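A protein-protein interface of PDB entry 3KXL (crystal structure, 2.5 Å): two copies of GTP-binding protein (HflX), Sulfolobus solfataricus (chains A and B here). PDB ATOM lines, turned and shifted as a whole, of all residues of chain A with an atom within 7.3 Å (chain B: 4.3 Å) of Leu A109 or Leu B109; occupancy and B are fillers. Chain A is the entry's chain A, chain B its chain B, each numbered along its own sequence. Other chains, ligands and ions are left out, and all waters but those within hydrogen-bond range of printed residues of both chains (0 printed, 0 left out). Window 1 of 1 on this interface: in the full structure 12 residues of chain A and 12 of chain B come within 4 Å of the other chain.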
ATOM      1  N   LEU A  91      -5.176   6.822   4.040  1.00  0.00           N
ATOM      2  CA  LEU A  91      -5.721   8.165   4.201  1.00  0.00           C
ATOM      3  C   LEU A  91      -6.691   8.493   3.073  1.00  0.00           C
ATOM      4  O   LEU A  91      -7.711   9.148   3.286  1.00  0.00           O
ATOM      5  CB  LEU A  91      -4.599   9.204   4.254  1.00  0.00           C
ATOM      6  CG  LEU A  91      -3.725   9.198   5.510  1.00  0.00           C
ATOM      7  CD1 LEU A  91      -2.616  10.231   5.393  1.00  0.00           C
ATOM      8  CD2 LEU A  91      -4.572   9.453   6.749  1.00  0.00           C
ATOM      9  N   ALA A 103     -13.364  14.212  10.944  1.00  0.00           N
ATOM     10  CA  ALA A 103     -12.702  13.140  10.211  1.00  0.00           C
ATOM     11  C   ALA A 103     -11.942  13.703   9.017  1.00  0.00           C
ATOM     12  O   ALA A 103     -10.743  13.470   8.866  1.00  0.00           O
ATOM     13  CB  ALA A 103     -13.712  12.100   9.759  1.00  0.00           C
ATOM     14  N   LYS A 104     -12.650  14.450   8.175  1.00  0.00           N
ATOM     15  CA  LYS A 104     -12.058  15.057   6.988  1.00  0.00           C
ATOM     16  C   LYS A 104     -10.812  15.872   7.328  1.00  0.00           C
ATOM     17  O   LYS A 104      -9.826  15.851   6.591  1.00  0.00           O
ATOM     18  CB  LYS A 104     -13.087  15.938   6.277  1.00  0.00           C
ATOM     19  CG  LYS A 104     -12.553  16.659   5.050  1.00  0.00           C
ATOM     20  CD  LYS A 104     -13.620  17.543   4.423  1.00  0.00           C
ATOM     21  CE  LYS A 104     -13.080  18.290   3.214  1.00  0.00           C
ATOM     22  NZ  LYS A 104     -12.602  17.361   2.153  1.00  0.00           N
ATOM     23  N   MET A 105     -10.861  16.587   8.447  1.00  0.00           N
ATOM     24  CA  MET A 105      -9.744  17.426   8.869  1.00  0.00           C
ATOM     25  C   MET A 105      -8.590  16.606   9.437  1.00  0.00           C
ATOM     26  O   MET A 105      -7.427  16.877   9.138  1.00  0.00           O
ATOM     27  CB  MET A 105     -10.209  18.469   9.888  1.00  0.00           C
ATOM     28  CG  MET A 105     -11.189  19.485   9.325  1.00  0.00           C
ATOM     29  SD  MET A 105     -11.688  20.712  10.547  1.00  0.00           S
ATOM     30  CE  MET A 105     -10.093  21.378  11.003  1.00  0.00           C
ATOM     31  N   GLN A 106      -8.913  15.612  10.259  1.00  0.00           N
ATOM     32  CA  GLN A 106      -7.902  14.713  10.805  1.00  0.00           C
ATOM     33  C   GLN A 106      -7.150  14.017   9.677  1.00  0.00           C
ATOM     34  O   GLN A 106      -5.929  13.871   9.726  1.00  0.00           O
ATOM     35  CB  GLN A 106      -8.543  13.669  11.724  1.00  0.00           C
ATOM     36  CG  GLN A 106      -8.988  14.203  13.077  1.00  0.00           C
ATOM     37  CD  GLN A 106      -7.823  14.502  14.003  1.00  0.00           C
ATOM     38  OE1 GLN A 106      -6.665  14.249  13.668  1.00  0.00           O
ATOM     39  NE2 GLN A 106      -8.125  15.040  15.179  1.00  0.00           N
ATOM     40  N   ILE A 107      -7.893  13.590   8.660  1.00  0.00           N
ATOM     41  CA  ILE A 107      -7.309  12.919   7.505  1.00  0.00           C
ATOM     42  C   ILE A 107      -6.384  13.854   6.736  1.00  0.00           C
ATOM     43  O   ILE A 107      -5.235  13.509   6.452  1.00  0.00           O
ATOM     44  CB  ILE A 107      -8.399  12.397   6.552  1.00  0.00           C
ATOM     45  CG1 ILE A 107      -9.299  11.393   7.274  1.00  0.00           C
ATOM     46  CG2 ILE A 107      -7.772  11.763   5.321  1.00  0.00           C
ATOM     47  CD1 ILE A 107     -10.546  11.026   6.502  1.00  0.00           C
ATOM     48  N   GLU A 108      -6.888  15.037   6.403  1.00  0.00           N
ATOM     49  CA  GLU A 108      -6.109  16.024   5.664  1.00  0.00           C
ATOM     50  C   GLU A 108      -4.883  16.472   6.457  1.00  0.00           C
ATOM     51  O   GLU A 108      -3.793  16.613   5.902  1.00  0.00           O
ATOM     52  CB  GLU A 108      -6.977  17.231   5.299  1.00  0.00           C
ATOM     53  CG  GLU A 108      -6.244  18.331   4.542  1.00  0.00           C
ATOM     54  CD  GLU A 108      -5.827  17.913   3.142  1.00  0.00           C
ATOM     55  OE1 GLU A 108      -5.973  16.720   2.801  1.00  0.00           O
ATOM     56  OE2 GLU A 108      -5.352  18.781   2.380  1.00  0.00           O
ATOM     57  N   LEU A 109      -5.067  16.689   7.755  1.00  0.00           N
ATOM     58  CA  LEU A 109      -3.968  17.084   8.629  1.00  0.00           C
ATOM     59  C   LEU A 109      -2.836  16.066   8.584  1.00  0.00           C
ATOM     60  O   LEU A 109      -1.676  16.420   8.372  1.00  0.00           O
ATOM     61  CB  LEU A 109      -4.458  17.248  10.069  1.00  0.00           C
ATOM     62  CG  LEU A 109      -3.378  17.545  11.112  1.00  0.00           C
ATOM     63  CD1 LEU A 109      -2.676  18.855  10.800  1.00  0.00           C
ATOM     64  CD2 LEU A 109      -3.974  17.574  12.512  1.00  0.00           C
ATOM     65  N   ALA A 110      -3.180  14.798   8.785  1.00  0.00           N
ATOM     66  CA  ALA A 110      -2.194  13.725   8.759  1.00  0.00           C
ATOM     67  C   ALA A 110      -1.563  13.595   7.377  1.00  0.00           C
ATOM     68  O   ALA A 110      -0.395  13.228   7.253  1.00  0.00           O
ATOM     69  CB  ALA A 110      -2.830  12.410   9.179  1.00  0.00           C
ATOM     70  N   ARG A 111      -2.340  13.898   6.343  1.00  0.00           N
ATOM     71  CA  ARG A 111      -1.852  13.806   4.973  1.00  0.00           C
ATOM     72  C   ARG A 111      -0.797  14.873   4.702  1.00  0.00           C
ATOM     73  O   ARG A 111       0.235  14.597   4.091  1.00  0.00           O
ATOM     74  CB  ARG A 111      -3.005  13.943   3.977  1.00  0.00           C
ATOM     75  CG  ARG A 111      -2.618  13.604   2.547  1.00  0.00           C
ATOM     76  CD  ARG A 111      -3.653  14.099   1.552  1.00  0.00           C
ATOM     77  NE  ARG A 111      -3.038  14.920   0.516  1.00  0.00           N
ATOM     78  CZ  ARG A 111      -2.899  16.238   0.595  1.00  0.00           C
ATOM     79  NH1 ARG A 111      -3.340  16.889   1.662  1.00  0.00           N
ATOM     80  NH2 ARG A 111      -2.323  16.908  -0.393  1.00  0.00           N
ATOM     81  N   LEU A 112      -1.064  16.092   5.160  1.00  0.00           N
ATOM     82  CA  LEU A 112      -0.131  17.198   4.987  1.00  0.00           C
ATOM     83  C   LEU A 112       1.135  16.987   5.812  1.00  0.00           C
ATOM     84  O   LEU A 112       2.231  17.347   5.383  1.00  0.00           O
ATOM     85  CB  LEU A 112      -0.794  18.523   5.365  1.00  0.00           C
ATOM     86  CG  LEU A 112      -1.988  18.956   4.512  1.00  0.00           C
ATOM     87  CD1 LEU A 112      -2.646  20.196   5.096  1.00  0.00           C
ATOM     88  CD2 LEU A 112      -1.561  19.199   3.072  1.00  0.00           C
ATOM     89  N   LYS A 113       0.979  16.406   6.997  1.00  0.00           N
ATOM     90  CA  LYS A 113       2.119  16.101   7.854  1.00  0.00           C
ATOM     91  C   LYS A 113       3.029  15.070   7.200  1.00  0.00           C
ATOM     92  O   LYS A 113       4.226  15.014   7.483  1.00  0.00           O
ATOM     93  CB  LYS A 113       1.653  15.579   9.216  1.00  0.00           C
ATOM     94  CG  LYS A 113       1.047  16.630  10.129  1.00  0.00           C
ATOM     95  CD  LYS A 113       0.763  16.047  11.505  1.00  0.00           C
ATOM     96  CE  LYS A 113       0.180  17.090  12.445  1.00  0.00           C
ATOM     97  NZ  LYS A 113      -0.043  16.537  13.810  1.00  0.00           N
ATOM     98  N   TYR A 114       2.452  14.253   6.326  1.00  0.00           N
ATOM     99  CA  TYR A 114       3.195  13.187   5.668  1.00  0.00           C
ATOM    100  C   TYR A 114       3.814  13.684   4.366  1.00  0.00           C
ATOM    101  O   TYR A 114       4.805  13.132   3.886  1.00  0.00           O
ATOM    102  CB  TYR A 114       2.279  11.990   5.405  1.00  0.00           C
ATOM    103  CG  TYR A 114       3.010  10.705   5.097  1.00  0.00           C
ATOM    104  CD1 TYR A 114       3.705  10.026   6.089  1.00  0.00           C
ATOM    105  CD2 TYR A 114       2.995  10.161   3.819  1.00  0.00           C
ATOM    106  CE1 TYR A 114       4.373   8.848   5.815  1.00  0.00           C
ATOM    107  CE2 TYR A 114       3.659   8.982   3.537  1.00  0.00           C
ATOM    108  CZ  TYR A 114       4.346   8.330   4.538  1.00  0.00           C
ATOM    109  OH  TYR A 114       5.009   7.156   4.264  1.00  0.00           O
ATOM    110  N   GLU A 115       3.224  14.735   3.802  1.00  0.00           N
ATOM    111  CA  GLU A 115       3.709  15.313   2.554  1.00  0.00           C
ATOM    112  C   GLU A 115       4.764  16.387   2.798  1.00  0.00           C
ATOM    113  O   GLU A 115       5.593  16.662   1.931  1.00  0.00           O
ATOM    114  CB  GLU A 115       2.547  15.899   1.749  1.00  0.00           C
ATOM    115  CG  GLU A 115       1.645  14.860   1.107  1.00  0.00           C
ATOM    116  CD  GLU A 115       2.311  14.149  -0.054  1.00  0.00           C
ATOM    117  OE1 GLU A 115       3.401  14.586  -0.478  1.00  0.00           O
ATOM    118  OE2 GLU A 115       1.740  13.155  -0.547  1.00  0.00           O
ATOM    119  N   LEU A 116       4.726  16.993   3.981  1.00  0.00           N
ATOM    120  CA  LEU A 116       5.655  18.067   4.321  1.00  0.00           C
ATOM    121  C   LEU A 116       7.120  17.638   4.192  1.00  0.00           C
ATOM    122  O   LEU A 116       7.902  18.308   3.519  1.00  0.00           O
ATOM    123  CB  LEU A 116       5.378  18.604   5.728  1.00  0.00           C
ATOM    124  CG  LEU A 116       5.255  20.123   5.860  1.00  0.00           C
ATOM    125  CD1 LEU A 116       5.324  20.530   7.323  1.00  0.00           C
ATOM    126  CD2 LEU A 116       6.339  20.824   5.058  1.00  0.00           C
ATOM    127  N   GLN A 243       0.996   7.270  12.800  1.00  0.00           N
ATOM    128  CA  GLN A 243       0.798   8.628  12.298  1.00  0.00           C
ATOM    129  C   GLN A 243      -0.628   8.898  11.818  1.00  0.00           C
ATOM    130  O   GLN A 243      -1.027  10.052  11.669  1.00  0.00           O
ATOM    131  CB  GLN A 243       1.799   8.946  11.183  1.00  0.00           C
ATOM    132  CG  GLN A 243       1.975   7.834  10.163  1.00  0.00           C
ATOM    133  CD  GLN A 243       3.251   7.043  10.381  1.00  0.00           C
ATOM    134  OE1 GLN A 243       4.353   7.571  10.230  1.00  0.00           O
ATOM    135  NE2 GLN A 243       3.107   5.771  10.732  1.00  0.00           N
ATOM    136  N   ALA A 247      -6.699   9.791  12.664  1.00  0.00           N
ATOM    137  CA  ALA A 247      -7.487   9.921  11.446  1.00  0.00           C
ATOM    138  C   ALA A 247      -8.448   8.746  11.293  1.00  0.00           C
ATOM    139  O   ALA A 247      -9.604   8.924  10.914  1.00  0.00           O
ATOM    140  CB  ALA A 247      -6.576  10.026  10.232  1.00  0.00           C
ATOM    141  N   MET B 105       0.877  24.501   2.300  1.00  0.00           N
ATOM    142  CA  MET B 105       0.713  23.391   3.230  1.00  0.00           C
ATOM    143  C   MET B 105       0.909  23.826   4.680  1.00  0.00           C
ATOM    144  O   MET B 105       0.096  23.504   5.546  1.00  0.00           O
ATOM    145  CB  MET B 105       1.679  22.259   2.880  1.00  0.00           C
ATOM    146  CG  MET B 105       1.459  21.672   1.495  1.00  0.00           C
ATOM    147  SD  MET B 105       2.714  20.458   1.045  1.00  0.00           S
ATOM    148  CE  MET B 105       2.588  19.318   2.419  1.00  0.00           C
ATOM    149  N   GLN B 106       1.990  24.554   4.938  1.00  0.00           N
ATOM    150  CA  GLN B 106       2.276  25.051   6.280  1.00  0.00           C
ATOM    151  C   GLN B 106       1.107  25.861   6.828  1.00  0.00           C
ATOM    152  O   GLN B 106       0.706  25.689   7.979  1.00  0.00           O
ATOM    153  CB  GLN B 106       3.547  25.904   6.279  1.00  0.00           C
ATOM    154  CG  GLN B 106       4.837  25.107   6.174  1.00  0.00           C
ATOM    155  CD  GLN B 106       5.172  24.363   7.453  1.00  0.00           C
ATOM    156  OE1 GLN B 106       4.435  24.431   8.437  1.00  0.00           O
ATOM    157  NE2 GLN B 106       6.292  23.650   7.447  1.00  0.00           N
ATOM    158  N   ILE B 107       0.565  26.744   5.997  1.00  0.00           N
ATOM    159  CA  ILE B 107      -0.556  27.587   6.394  1.00  0.00           C
ATOM    160  C   ILE B 107      -1.787  26.747   6.711  1.00  0.00           C
ATOM    161  O   ILE B 107      -2.451  26.960   7.725  1.00  0.00           O
ATOM    162  CB  ILE B 107      -0.906  28.605   5.296  1.00  0.00           C
ATOM    163  CG1 ILE B 107       0.300  29.498   4.999  1.00  0.00           C
ATOM    164  CG2 ILE B 107      -2.103  29.445   5.712  1.00  0.00           C
ATOM    165  CD1 ILE B 107       0.145  30.336   3.751  1.00  0.00           C
ATOM    166  N   GLU B 108      -2.086  25.790   5.839  1.00  0.00           N
ATOM    167  CA  GLU B 108      -3.237  24.916   6.026  1.00  0.00           C
ATOM    168  C   GLU B 108      -3.062  24.036   7.261  1.00  0.00           C
ATOM    169  O   GLU B 108      -4.021  23.767   7.983  1.00  0.00           O
ATOM    170  CB  GLU B 108      -3.466  24.052   4.783  1.00  0.00           C
ATOM    171  CG  GLU B 108      -4.692  23.155   4.857  1.00  0.00           C
ATOM    172  CD  GLU B 108      -5.992  23.936   4.919  1.00  0.00           C
ATOM    173  OE1 GLU B 108      -5.950  25.181   4.835  1.00  0.00           O
ATOM    174  OE2 GLU B 108      -7.061  23.302   5.051  1.00  0.00           O
ATOM    175  N   LEU B 109      -1.831  23.592   7.498  1.00  0.00           N
ATOM    176  CA  LEU B 109      -1.516  22.790   8.675  1.00  0.00           C
ATOM    177  C   LEU B 109      -1.861  23.538   9.956  1.00  0.00           C
ATOM    178  O   LEU B 109      -2.560  23.014  10.822  1.00  0.00           O
ATOM    179  CB  LEU B 109      -0.035  22.404   8.681  1.00  0.00           C
ATOM    180  CG  LEU B 109       0.365  21.203   7.824  1.00  0.00           C
ATOM    181  CD1 LEU B 109       1.874  21.138   7.658  1.00  0.00           C
ATOM    182  CD2 LEU B 109      -0.170  19.916   8.435  1.00  0.00           C
ATOM    183  N   ALA B 110      -1.366  24.766  10.066  1.00  0.00           N
ATOM    184  CA  ALA B 110      -1.641  25.600  11.229  1.00  0.00           C
ATOM    185  C   ALA B 110      -3.136  25.855  11.378  1.00  0.00           C
ATOM    186  O   ALA B 110      -3.658  25.908  12.491  1.00  0.00           O
ATOM    187  CB  ALA B 110      -0.886  26.916  11.127  1.00  0.00           C
ATOM    188  N   ARG B 111      -3.820  26.011  10.249  1.00  0.00           N
ATOM    189  CA  ARG B 111      -5.256  26.265  10.254  1.00  0.00           C
ATOM    190  C   ARG B 111      -6.032  25.065  10.788  1.00  0.00           C
ATOM    191  O   ARG B 111      -6.993  25.221  11.543  1.00  0.00           O
ATOM    192  CB  ARG B 111      -5.746  26.623   8.851  1.00  0.00           C
ATOM    193  CG  ARG B 111      -7.255  26.751   8.746  1.00  0.00           C
ATOM    194  CD  ARG B 111      -7.698  26.949   7.308  1.00  0.00           C
ATOM    195  NE  ARG B 111      -9.137  26.758   7.160  1.00  0.00           N
ATOM    196  CZ  ARG B 111      -9.710  25.582   6.924  1.00  0.00           C
ATOM    197  NH1 ARG B 111      -8.965  24.491   6.809  1.00  0.00           N
ATOM    198  NH2 ARG B 111     -11.027  25.495   6.804  1.00  0.00           N
ATOM    199  N   LEU B 112      -5.611  23.869  10.392  1.00  0.00           N
ATOM    200  CA  LEU B 112      -6.261  22.644  10.841  1.00  0.00           C
ATOM    201  C   LEU B 112      -6.009  22.396  12.326  1.00  0.00           C
ATOM    202  O   LEU B 112      -6.937  22.107  13.080  1.00  0.00           O
ATOM    203  CB  LEU B 112      -5.793  21.448  10.011  1.00  0.00           C
ATOM    204  CG  LEU B 112      -6.169  21.471   8.527  1.00  0.00           C
ATOM    205  CD1 LEU B 112      -5.572  20.277   7.800  1.00  0.00           C
ATOM    206  CD2 LEU B 112      -7.680  21.507   8.355  1.00  0.00           C
ATOM    207  N   LYS B 113      -4.753  22.516  12.741  1.00  0.00           N
ATOM    208  CA  LYS B 113      -4.390  22.329  14.143  1.00  0.00           C
ATOM    209  C   LYS B 113      -5.139  23.307  15.044  1.00  0.00           C
ATOM    210  O   LYS B 113      -5.312  23.058  16.236  1.00  0.00           O
ATOM    211  CB  LYS B 113      -2.883  22.501  14.341  1.00  0.00           C
ATOM    212  CG  LYS B 113      -2.032  21.454  13.645  1.00  0.00           C
ATOM    213  CD  LYS B 113      -0.555  21.678  13.934  1.00  0.00           C
ATOM    214  CE  LYS B 113       0.313  20.653  13.223  1.00  0.00           C
ATOM    215  NZ  LYS B 113       1.761  20.880  13.480  1.00  0.00           N
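The guanidinium group of Arg A111 is in salt-bridge range of the side-chain carboxylate of Glu A108, at 2.9 Å.
The side-chain carboxylate of Glu B108 is in salt-bridge range of the guanidinium group of Arg B111 (2.9 Å).
Among the printed residues, pairs that only touch across the chains: Met A105 with Leu B112 (3.6 Å), Glu A108 with Leu B112 (3.9 Å), Leu A109 with Leu B109 (3.6 Å), Leu A109 with Leu B112 (3.6 Å), Leu A109 with Lys B113 (3.9 Å), Leu A112 with Met B105 (3.6 Å), Leu A112 with Glu B108 (3.6 Å), Leu A112 with Leu B109 (3.4 Å), Leu A112 with Leu B112 (3.98 Å), Lys A113 with Leu B109 (3.9 Å), Lys A113 with Lys B113 (3.6 Å), Glu A115 with Met B105 (3.5 Å), Leu A116 with Met B105 (3.5 Å), Leu A116 with Gln B106 (3.3 Å) and Leu A116 with Leu B109 (3.5 Å).
Of the printed residues of chain B, Leu A109 touches Leu B109, Leu B112 and Lys B113.
Printed residues of chain B within 4 Å of Lys A113: Leu B109 (3.9 Å) and Lys B113 (3.6 Å).
Of the printed residues of chain A, Met B105 touches Leu A112 (3.6 Å), Glu A115 (3.5 Å) and Leu A116 (3.5 Å).
Printed residues of chain A within 4 Å of Glu B108: Leu A112 (3.6 Å).
Leu B109 touches just these residues of chain A: Leu A109 (3.6 Å), Leu A112 (3.4 Å), Lys A113 (3.9 Å) and Leu A116 (3.5 Å).
The nearest printed residue of chain B that does not touch Leu A109 is Glu B108 (5.8 Å).
The nearest printed residue of chain A that does not touch Met B105 is Arg A111 (5.5 Å).
Printed residues of chain A that touch a printed residue of chain B: Met A105, Glu A108, Leu A109, Leu A112, Lys A113, Glu A115 and Leu A116.
Of the 9 printed residues of chain B, 6 touch a printed residue of chain A.
Among the printed residues, 15 pairs touch across the chains.
Among the printed residues, no Asp or Glu carboxylate lies within 4 Å of a Lys or Arg side-chain nitrogen of the other chain.
Glu A108 touches Leu B112, and with the chains exchanged Leu A112 touches Glu B108.
Leu A109 touches its own counterpart, Leu B109.
Leu B112 touches its own counterpart, Leu A112.
Lys A113 touches its own counterpart, Lys B113.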
